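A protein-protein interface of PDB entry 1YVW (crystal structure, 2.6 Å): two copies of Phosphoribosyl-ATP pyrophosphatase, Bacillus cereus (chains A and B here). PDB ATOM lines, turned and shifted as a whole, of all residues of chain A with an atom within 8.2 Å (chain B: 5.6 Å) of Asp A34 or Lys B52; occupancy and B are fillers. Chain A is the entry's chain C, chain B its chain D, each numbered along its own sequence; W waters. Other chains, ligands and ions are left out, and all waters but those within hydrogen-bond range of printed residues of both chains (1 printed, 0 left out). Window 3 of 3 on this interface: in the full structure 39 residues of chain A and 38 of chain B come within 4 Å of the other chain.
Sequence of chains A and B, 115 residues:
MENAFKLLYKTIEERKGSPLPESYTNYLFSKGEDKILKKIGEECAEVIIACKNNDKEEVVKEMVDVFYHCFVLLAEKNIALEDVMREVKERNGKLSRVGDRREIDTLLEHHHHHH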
ATOM      1  N   LEU A  28       5.903  10.143  -3.081  1.00  0.00           N
ATOM      2  CA  LEU A  28       6.389  11.451  -3.500  1.00  0.00           C
ATOM      3  C   LEU A  28       5.484  12.083  -4.539  1.00  0.00           C
ATOM      4  O   LEU A  28       5.145  13.265  -4.422  1.00  0.00           O
ATOM      5  CB  LEU A  28       7.820  11.357  -4.028  1.00  0.00           C
ATOM      6  CG  LEU A  28       8.905  11.099  -2.975  1.00  0.00           C
ATOM      7  CD1 LEU A  28      10.240  10.992  -3.665  1.00  0.00           C
ATOM      8  CD2 LEU A  28       8.919  12.215  -1.922  1.00  0.00           C
ATOM      9  N   LYS A  31       2.218  13.228  -2.860  1.00  0.00           N
ATOM     10  CA  LYS A  31       2.371  14.454  -2.066  1.00  0.00           C
ATOM     11  C   LYS A  31       2.716  15.630  -2.975  1.00  0.00           C
ATOM     12  O   LYS A  31       2.457  16.773  -2.645  1.00  0.00           O
ATOM     13  CB  LYS A  31       3.432  14.291  -0.968  1.00  0.00           C
ATOM     14  CG  LYS A  31       3.063  13.312   0.136  1.00  0.00           C
ATOM     15  CD  LYS A  31       1.821  13.756   0.889  1.00  0.00           C
ATOM     16  CE  LYS A  31       1.373  12.701   1.896  1.00  0.00           C
ATOM     17  NZ  LYS A  31       0.059  13.035   2.538  1.00  0.00           N
ATOM     18  N   GLY A  32       3.329  15.336  -4.113  1.00  0.00           N
ATOM     19  CA  GLY A  32       3.660  16.377  -5.061  1.00  0.00           C
ATOM     20  C   GLY A  32       4.962  17.146  -4.956  1.00  0.00           C
ATOM     21  O   GLY A  32       5.863  16.869  -4.147  1.00  0.00           O
ATOM     22  N   GLU A  33       5.017  18.144  -5.828  1.00  0.00           N
ATOM     23  CA  GLU A  33       6.130  19.062  -6.011  1.00  0.00           C
ATOM     24  C   GLU A  33       6.794  19.587  -4.731  1.00  0.00           C
ATOM     25  O   GLU A  33       8.002  19.476  -4.568  1.00  0.00           O
ATOM     26  CB  GLU A  33       5.601  20.214  -6.861  1.00  0.00           C
ATOM     27  CG  GLU A  33       6.577  21.255  -7.282  1.00  0.00           C
ATOM     28  CD  GLU A  33       5.870  22.421  -7.930  1.00  0.00           C
ATOM     29  OE1 GLU A  33       4.901  22.934  -7.335  1.00  0.00           O
ATOM     30  OE2 GLU A  33       6.279  22.813  -9.037  1.00  0.00           O
ATOM     31  N   ASP A  34       5.993  20.155  -3.838  1.00  0.00           N
ATOM     32  CA  ASP A  34       6.486  20.720  -2.591  1.00  0.00           C
ATOM     33  C   ASP A  34       7.198  19.725  -1.671  1.00  0.00           C
ATOM     34  O   ASP A  34       8.148  20.083  -0.979  1.00  0.00           O
ATOM     35  CB  ASP A  34       5.352  21.432  -1.841  1.00  0.00           C
ATOM     36  CG  ASP A  34       4.839  22.686  -2.587  1.00  0.00           C
ATOM     37  OD1 ASP A  34       5.368  23.030  -3.664  1.00  0.00           O
ATOM     38  OD2 ASP A  34       3.895  23.331  -2.069  1.00  0.00           O
ATOM     39  N   LYS A  35       6.757  18.470  -1.693  1.00  0.00           N
ATOM     40  CA  LYS A  35       7.376  17.447  -0.879  1.00  0.00           C
ATOM     41  C   LYS A  35       8.749  17.110  -1.461  1.00  0.00           C
ATOM     42  O   LYS A  35       9.730  17.011  -0.738  1.00  0.00           O
ATOM     43  CB  LYS A  35       6.505  16.189  -0.851  1.00  0.00           C
ATOM     44  CG  LYS A  35       6.985  15.106   0.110  1.00  0.00           C
ATOM     45  CD  LYS A  35       6.798  15.547   1.547  1.00  0.00           C
ATOM     46  CE  LYS A  35       7.099  14.427   2.527  1.00  0.00           C
ATOM     47  NZ  LYS A  35       6.868  14.864   3.940  1.00  0.00           N
ATOM     48  N   ILE A  36       8.805  16.954  -2.770  1.00  0.00           N
ATOM     49  CA  ILE A  36      10.044  16.606  -3.461  1.00  0.00           C
ATOM     50  C   ILE A  36      11.107  17.685  -3.291  1.00  0.00           C
ATOM     51  O   ILE A  36      12.271  17.389  -3.031  1.00  0.00           O
ATOM     52  CB  ILE A  36       9.782  16.361  -4.973  1.00  0.00           C
ATOM     53  CG1 ILE A  36       8.653  15.333  -5.137  1.00  0.00           C
ATOM     54  CG2 ILE A  36      11.053  15.904  -5.673  1.00  0.00           C
ATOM     55  CD1 ILE A  36       8.126  15.203  -6.545  1.00  0.00           C
ATOM     56  N   LEU A  37      10.671  18.938  -3.393  1.00  0.00           N
ATOM     57  CA  LEU A  37      11.542  20.088  -3.257  1.00  0.00           C
ATOM     58  C   LEU A  37      12.128  20.171  -1.856  1.00  0.00           C
ATOM     59  O   LEU A  37      13.307  20.487  -1.692  1.00  0.00           O
ATOM     60  CB  LEU A  37      10.769  21.364  -3.613  1.00  0.00           C
ATOM     61  CG  LEU A  37      10.369  21.461  -5.093  1.00  0.00           C
ATOM     62  CD1 LEU A  37       9.496  22.673  -5.336  1.00  0.00           C
ATOM     63  CD2 LEU A  37      11.599  21.468  -6.001  1.00  0.00           C
ATOM     64  N   LYS A  38      11.311  19.859  -0.851  1.00  0.00           N
ATOM     65  CA  LYS A  38      11.764  19.864   0.537  1.00  0.00           C
ATOM     66  C   LYS A  38      12.838  18.807   0.714  1.00  0.00           C
ATOM     67  O   LYS A  38      13.825  19.037   1.401  1.00  0.00           O
ATOM     68  CB  LYS A  38      10.603  19.588   1.494  1.00  0.00           C
ATOM     69  CG  LYS A  38       9.690  20.785   1.664  1.00  0.00           C
ATOM     70  CD  LYS A  38       8.314  20.420   2.224  1.00  0.00           C
ATOM     71  CE  LYS A  38       7.385  21.637   2.230  1.00  0.00           C
ATOM     72  NZ  LYS A  38       5.998  21.275   2.617  1.00  0.00           N
ATOM     73  N   LYS A  39      12.639  17.660   0.073  1.00  0.00           N
ATOM     74  CA  LYS A  39      13.592  16.563   0.130  1.00  0.00           C
ATOM     75  C   LYS A  39      14.927  16.953  -0.494  1.00  0.00           C
ATOM     76  O   LYS A  39      15.978  16.633   0.047  1.00  0.00           O
ATOM     77  CB  LYS A  39      13.029  15.331  -0.574  1.00  0.00           C
ATOM     78  CG  LYS A  39      11.956  14.627   0.227  1.00  0.00           C
ATOM     79  CD  LYS A  39      12.540  14.012   1.483  1.00  0.00           C
ATOM     80  CE  LYS A  39      11.501  13.204   2.234  1.00  0.00           C
ATOM     81  NZ  LYS A  39      12.107  12.574   3.440  1.00  0.00           N
ATOM     82  N   ILE A  40      14.868  17.673  -1.615  1.00  0.00           N
ATOM     83  CA  ILE A  40      16.062  18.106  -2.306  1.00  0.00           C
ATOM     84  C   ILE A  40      16.876  19.066  -1.434  1.00  0.00           C
ATOM     85  O   ILE A  40      18.106  18.941  -1.360  1.00  0.00           O
ATOM     86  CB  ILE A  40      15.735  18.742  -3.692  1.00  0.00           C
ATOM     87  CG1 ILE A  40      15.238  17.649  -4.656  1.00  0.00           C
ATOM     88  CG2 ILE A  40      16.962  19.489  -4.273  1.00  0.00           C
ATOM     89  CD1 ILE A  40      14.663  18.162  -5.977  1.00  0.00           C
ATOM     90  N   GLY A  41      16.179  19.966  -0.736  1.00  0.00           N
ATOM     91  CA  GLY A  41      16.838  20.932   0.121  1.00  0.00           C
ATOM     92  C   GLY A  41      17.502  20.263   1.301  1.00  0.00           C
ATOM     93  O   GLY A  41      18.636  20.579   1.658  1.00  0.00           O
ATOM     94  N   LEU A  73      11.473  14.758  -9.458  1.00  0.00           N
ATOM     95  CA  LEU A  73      10.954  16.099  -9.721  1.00  0.00           C
ATOM     96  C   LEU A  73      10.747  16.319 -11.238  1.00  0.00           C
ATOM     97  O   LEU A  73       9.760  16.919 -11.656  1.00  0.00           O
ATOM     98  CB  LEU A  73      11.903  17.173  -9.163  1.00  0.00           C
ATOM     99  CG  LEU A  73      11.396  18.619  -9.314  1.00  0.00           C
ATOM    100  CD1 LEU A  73      10.283  18.876  -8.321  1.00  0.00           C
ATOM    101  CD2 LEU A  73      12.515  19.617  -9.133  1.00  0.00           C
ATOM    102  N   GLU A  76       7.690  14.443 -12.280  1.00  0.00           N
ATOM    103  CA  GLU A  76       6.533  15.133 -11.721  1.00  0.00           C
ATOM    104  C   GLU A  76       6.160  16.403 -12.508  1.00  0.00           C
ATOM    105  O   GLU A  76       4.984  16.707 -12.688  1.00  0.00           O
ATOM    106  CB  GLU A  76       6.805  15.483 -10.249  1.00  0.00           C
ATOM    107  CG  GLU A  76       5.778  16.406  -9.596  1.00  0.00           C
ATOM    108  CD  GLU A  76       4.421  15.753  -9.367  1.00  0.00           C
ATOM    109  OE1 GLU A  76       4.303  14.506  -9.462  1.00  0.00           O
ATOM    110  OE2 GLU A  76       3.470  16.505  -9.069  1.00  0.00           O
ATOM    111  N   LYS A  77       7.168  17.156 -12.947  1.00  0.00           N
ATOM    112  CA  LYS A  77       6.949  18.380 -13.705  1.00  0.00           C
ATOM    113  C   LYS A  77       6.866  18.100 -15.213  1.00  0.00           C
ATOM    114  O   LYS A  77       6.768  19.028 -16.019  1.00  0.00           O
ATOM    115  CB  LYS A  77       8.080  19.371 -13.432  1.00  0.00           C
ATOM    116  CG  LYS A  77       8.227  19.761 -11.988  1.00  0.00           C
ATOM    117  CD  LYS A  77       7.024  20.563 -11.508  1.00  0.00           C
ATOM    118  CE  LYS A  77       6.934  21.905 -12.220  1.00  0.00           C
ATOM    119  NZ  LYS A  77       5.767  22.679 -11.738  1.00  0.00           N
ATOM    120  N   VAL B  47      16.870  25.849  -7.996  1.00  0.00           N
ATOM    121  CA  VAL B  47      16.069  24.797  -8.584  1.00  0.00           C
ATOM    122  C   VAL B  47      14.651  24.836  -7.992  1.00  0.00           C
ATOM    123  O   VAL B  47      13.663  24.675  -8.703  1.00  0.00           O
ATOM    124  CB  VAL B  47      16.692  23.400  -8.346  1.00  0.00           C
ATOM    125  CG1 VAL B  47      15.651  22.295  -8.622  1.00  0.00           C
ATOM    126  CG2 VAL B  47      17.911  23.192  -9.238  1.00  0.00           C
ATOM    127  N   ILE B  48      14.574  25.058  -6.682  1.00  0.00           N
ATOM    128  CA  ILE B  48      13.301  25.132  -5.980  1.00  0.00           C
ATOM    129  C   ILE B  48      12.476  26.305  -6.521  1.00  0.00           C
ATOM    130  O   ILE B  48      11.312  26.134  -6.895  1.00  0.00           O
ATOM    131  CB  ILE B  48      13.522  25.261  -4.437  1.00  0.00           C
ATOM    132  CG1 ILE B  48      14.081  23.933  -3.895  1.00  0.00           C
ATOM    133  CG2 ILE B  48      12.237  25.572  -3.732  1.00  0.00           C
ATOM    134  CD1 ILE B  48      14.537  23.938  -2.433  1.00  0.00           C
ATOM    135  N   ILE B  49      13.105  27.478  -6.581  1.00  0.00           N
ATOM    136  CA  ILE B  49      12.481  28.699  -7.067  1.00  0.00           C
ATOM    137  C   ILE B  49      12.021  28.546  -8.521  1.00  0.00           C
ATOM    138  O   ILE B  49      10.892  28.897  -8.863  1.00  0.00           O
ATOM    139  CB  ILE B  49      13.453  29.899  -6.957  1.00  0.00           C
ATOM    140  CG1 ILE B  49      13.744  30.187  -5.486  1.00  0.00           C
ATOM    141  CG2 ILE B  49      12.875  31.160  -7.631  1.00  0.00           C
ATOM    142  CD1 ILE B  49      14.919  31.083  -5.256  1.00  0.00           C
ATOM    143  N   ALA B  50      12.894  27.991  -9.361  1.00  0.00           N
ATOM    144  CA  ALA B  50      12.577  27.779 -10.765  1.00  0.00           C
ATOM    145  C   ALA B  50      11.400  26.821 -10.937  1.00  0.00           C
ATOM    146  O   ALA B  50      10.530  27.043 -11.777  1.00  0.00           O
ATOM    147  CB  ALA B  50      13.796  27.248 -11.509  1.00  0.00           C
ATOM    148  N   CYS B  51      11.377  25.761 -10.136  1.00  0.00           N
ATOM    149  CA  CYS B  51      10.312  24.787 -10.205  1.00  0.00           C
ATOM    150  C   CYS B  51       8.955  25.391  -9.824  1.00  0.00           C
ATOM    151  O   CYS B  51       7.948  25.128 -10.487  1.00  0.00           O
ATOM    152  CB  CYS B  51      10.636  23.579  -9.326  1.00  0.00           C
ATOM    153  SG  CYS B  51       9.360  22.325  -9.380  1.00  0.00           S
ATOM    154  N   LYS B  52       8.946  26.230  -8.791  1.00  0.00           N
ATOM    155  CA  LYS B  52       7.729  26.885  -8.339  1.00  0.00           C
ATOM    156  C   LYS B  52       7.246  27.935  -9.334  1.00  0.00           C
ATOM    157  O   LYS B  52       6.063  28.291  -9.350  1.00  0.00           O
ATOM    158  CB  LYS B  52       7.926  27.517  -6.963  1.00  0.00           C
ATOM    159  CG  LYS B  52       8.186  26.511  -5.850  1.00  0.00           C
ATOM    160  CD  LYS B  52       7.043  25.530  -5.701  1.00  0.00           C
ATOM    161  CE  LYS B  52       5.798  26.214  -5.191  1.00  0.00           C
ATOM    162  NZ  LYS B  52       4.670  25.267  -5.132  1.00  0.00           N
ATOM    163  N   ASN B  53       8.169  28.437 -10.150  1.00  0.00           N
ATOM    164  CA  ASN B  53       7.866  29.432 -11.176  1.00  0.00           C
ATOM    165  C   ASN B  53       7.357  28.741 -12.433  1.00  0.00           C
ATOM    166  O   ASN B  53       6.917  29.398 -13.379  1.00  0.00           O
ATOM    167  CB  ASN B  53       9.116  30.250 -11.538  1.00  0.00           C
ATOM    168  CG  ASN B  53       9.385  31.376 -10.566  1.00  0.00           C
ATOM    169  OD1 ASN B  53       8.483  31.849  -9.889  1.00  0.00           O
ATOM    170  ND2 ASN B  53      10.631  31.823 -10.506  1.00  0.00           N
ATOM    171  N   ASN B  54       7.455  27.408 -12.437  1.00  0.00           N
ATOM    172  CA  ASN B  54       7.027  26.572 -13.558  1.00  0.00           C
ATOM    173  C   ASN B  54       7.835  26.832 -14.816  1.00  0.00           C
ATOM    174  O   ASN B  54       7.374  26.600 -15.930  1.00  0.00           O
ATOM    175  CB  ASN B  54       5.533  26.746 -13.838  1.00  0.00           C
ATOM    176  CG  ASN B  54       4.674  26.109 -12.778  1.00  0.00           C
ATOM    177  OD1 ASN B  54       4.844  24.935 -12.452  1.00  0.00           O
ATOM    178  ND2 ASN B  54       3.736  26.878 -12.229  1.00  0.00           N
HETATM  179  O   HOH W   1       5.950  23.364 -14.932  1.00  0.00           O
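NZ of Lys A77 sits at hydrogen-bond distance from OD1 of Asn B54 (2.5 Å).
The side-chain carboxylate (OE2) of Glu A33 lies within hydrogen-bond range of the side-chain sulfur (SG) of Cys B51.
NZ of Lys B52 lies within salt-bridge range of OD1 of Asp A34 (2.8 Å).
The side-chain carboxylate (OE1) of Glu A33 lies within salt-bridge range of the side-chain amino group (NZ) of Lys B52 (3.2 Å).
OE2 of Glu A33 lies within salt-bridge range of NZ of Lys A77 (2.8 Å).
Among the printed residues, merely in contact across the chains: Lys A77 with Cys B51 (3.5 Å), Leu A73 with Cys B51 (3.7 Å), Leu A37 with Ile B48 (3.7 Å) and Leu A37 with Lys B52 (3.8 Å).
Lys B52 touches three residues of chain A.
Of the printed residues of chain B, Leu A73 touches Cys B51 (3.7 Å).
Of the printed residues of chain A, Asn B54 touches Lys A77.
Of the printed residues of chain B, Lys A77 touches Cys B51 and Asn B54.
The nearest printed residue of chain B that does not touch Asp A34 is Cys B51 (6.8 Å).
The nearest residue of chain A that does not touch Lys B52 is Lys A77 (5.6 Å).
Of the 8 printed residues of chain B, 4 touch a printed residue of chain A.
Printed residues of chain B that touch a printed residue of chain A: Ile B48, Cys B51, Lys B52 and Asn B54.
Of the 15 printed residues of chain A, 5 touch a printed residue of chain B.
Printed residues of chain A that touch a printed residue of chain B: Glu A33, Asp A34, Leu A37, Leu A73 and Lys A77.
Hydrophobic or aromatic side chains of chain A within 4 Å of the printed part of chain B: Leu A37 and Leu A73.
Among the printed residues, Asp or Glu carboxylates within 4 Å of a Lys or Arg side-chain nitrogen of the other chain: Glu A33 with Lys B52 (3.2 Å) and Asp A34 with Lys B52 (2.8 Å).
No position is printed for both chains.
Of the 8 pairs that touch across the chains among the printed residues, none has its exchanged pair printed and touching as well.
Water W1 bridges the side-chain amide oxygen (OD1) of Asn B54 (3.1 Å) and the side-chain amino group (NZ) of Lys A77 (3.3 Å).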
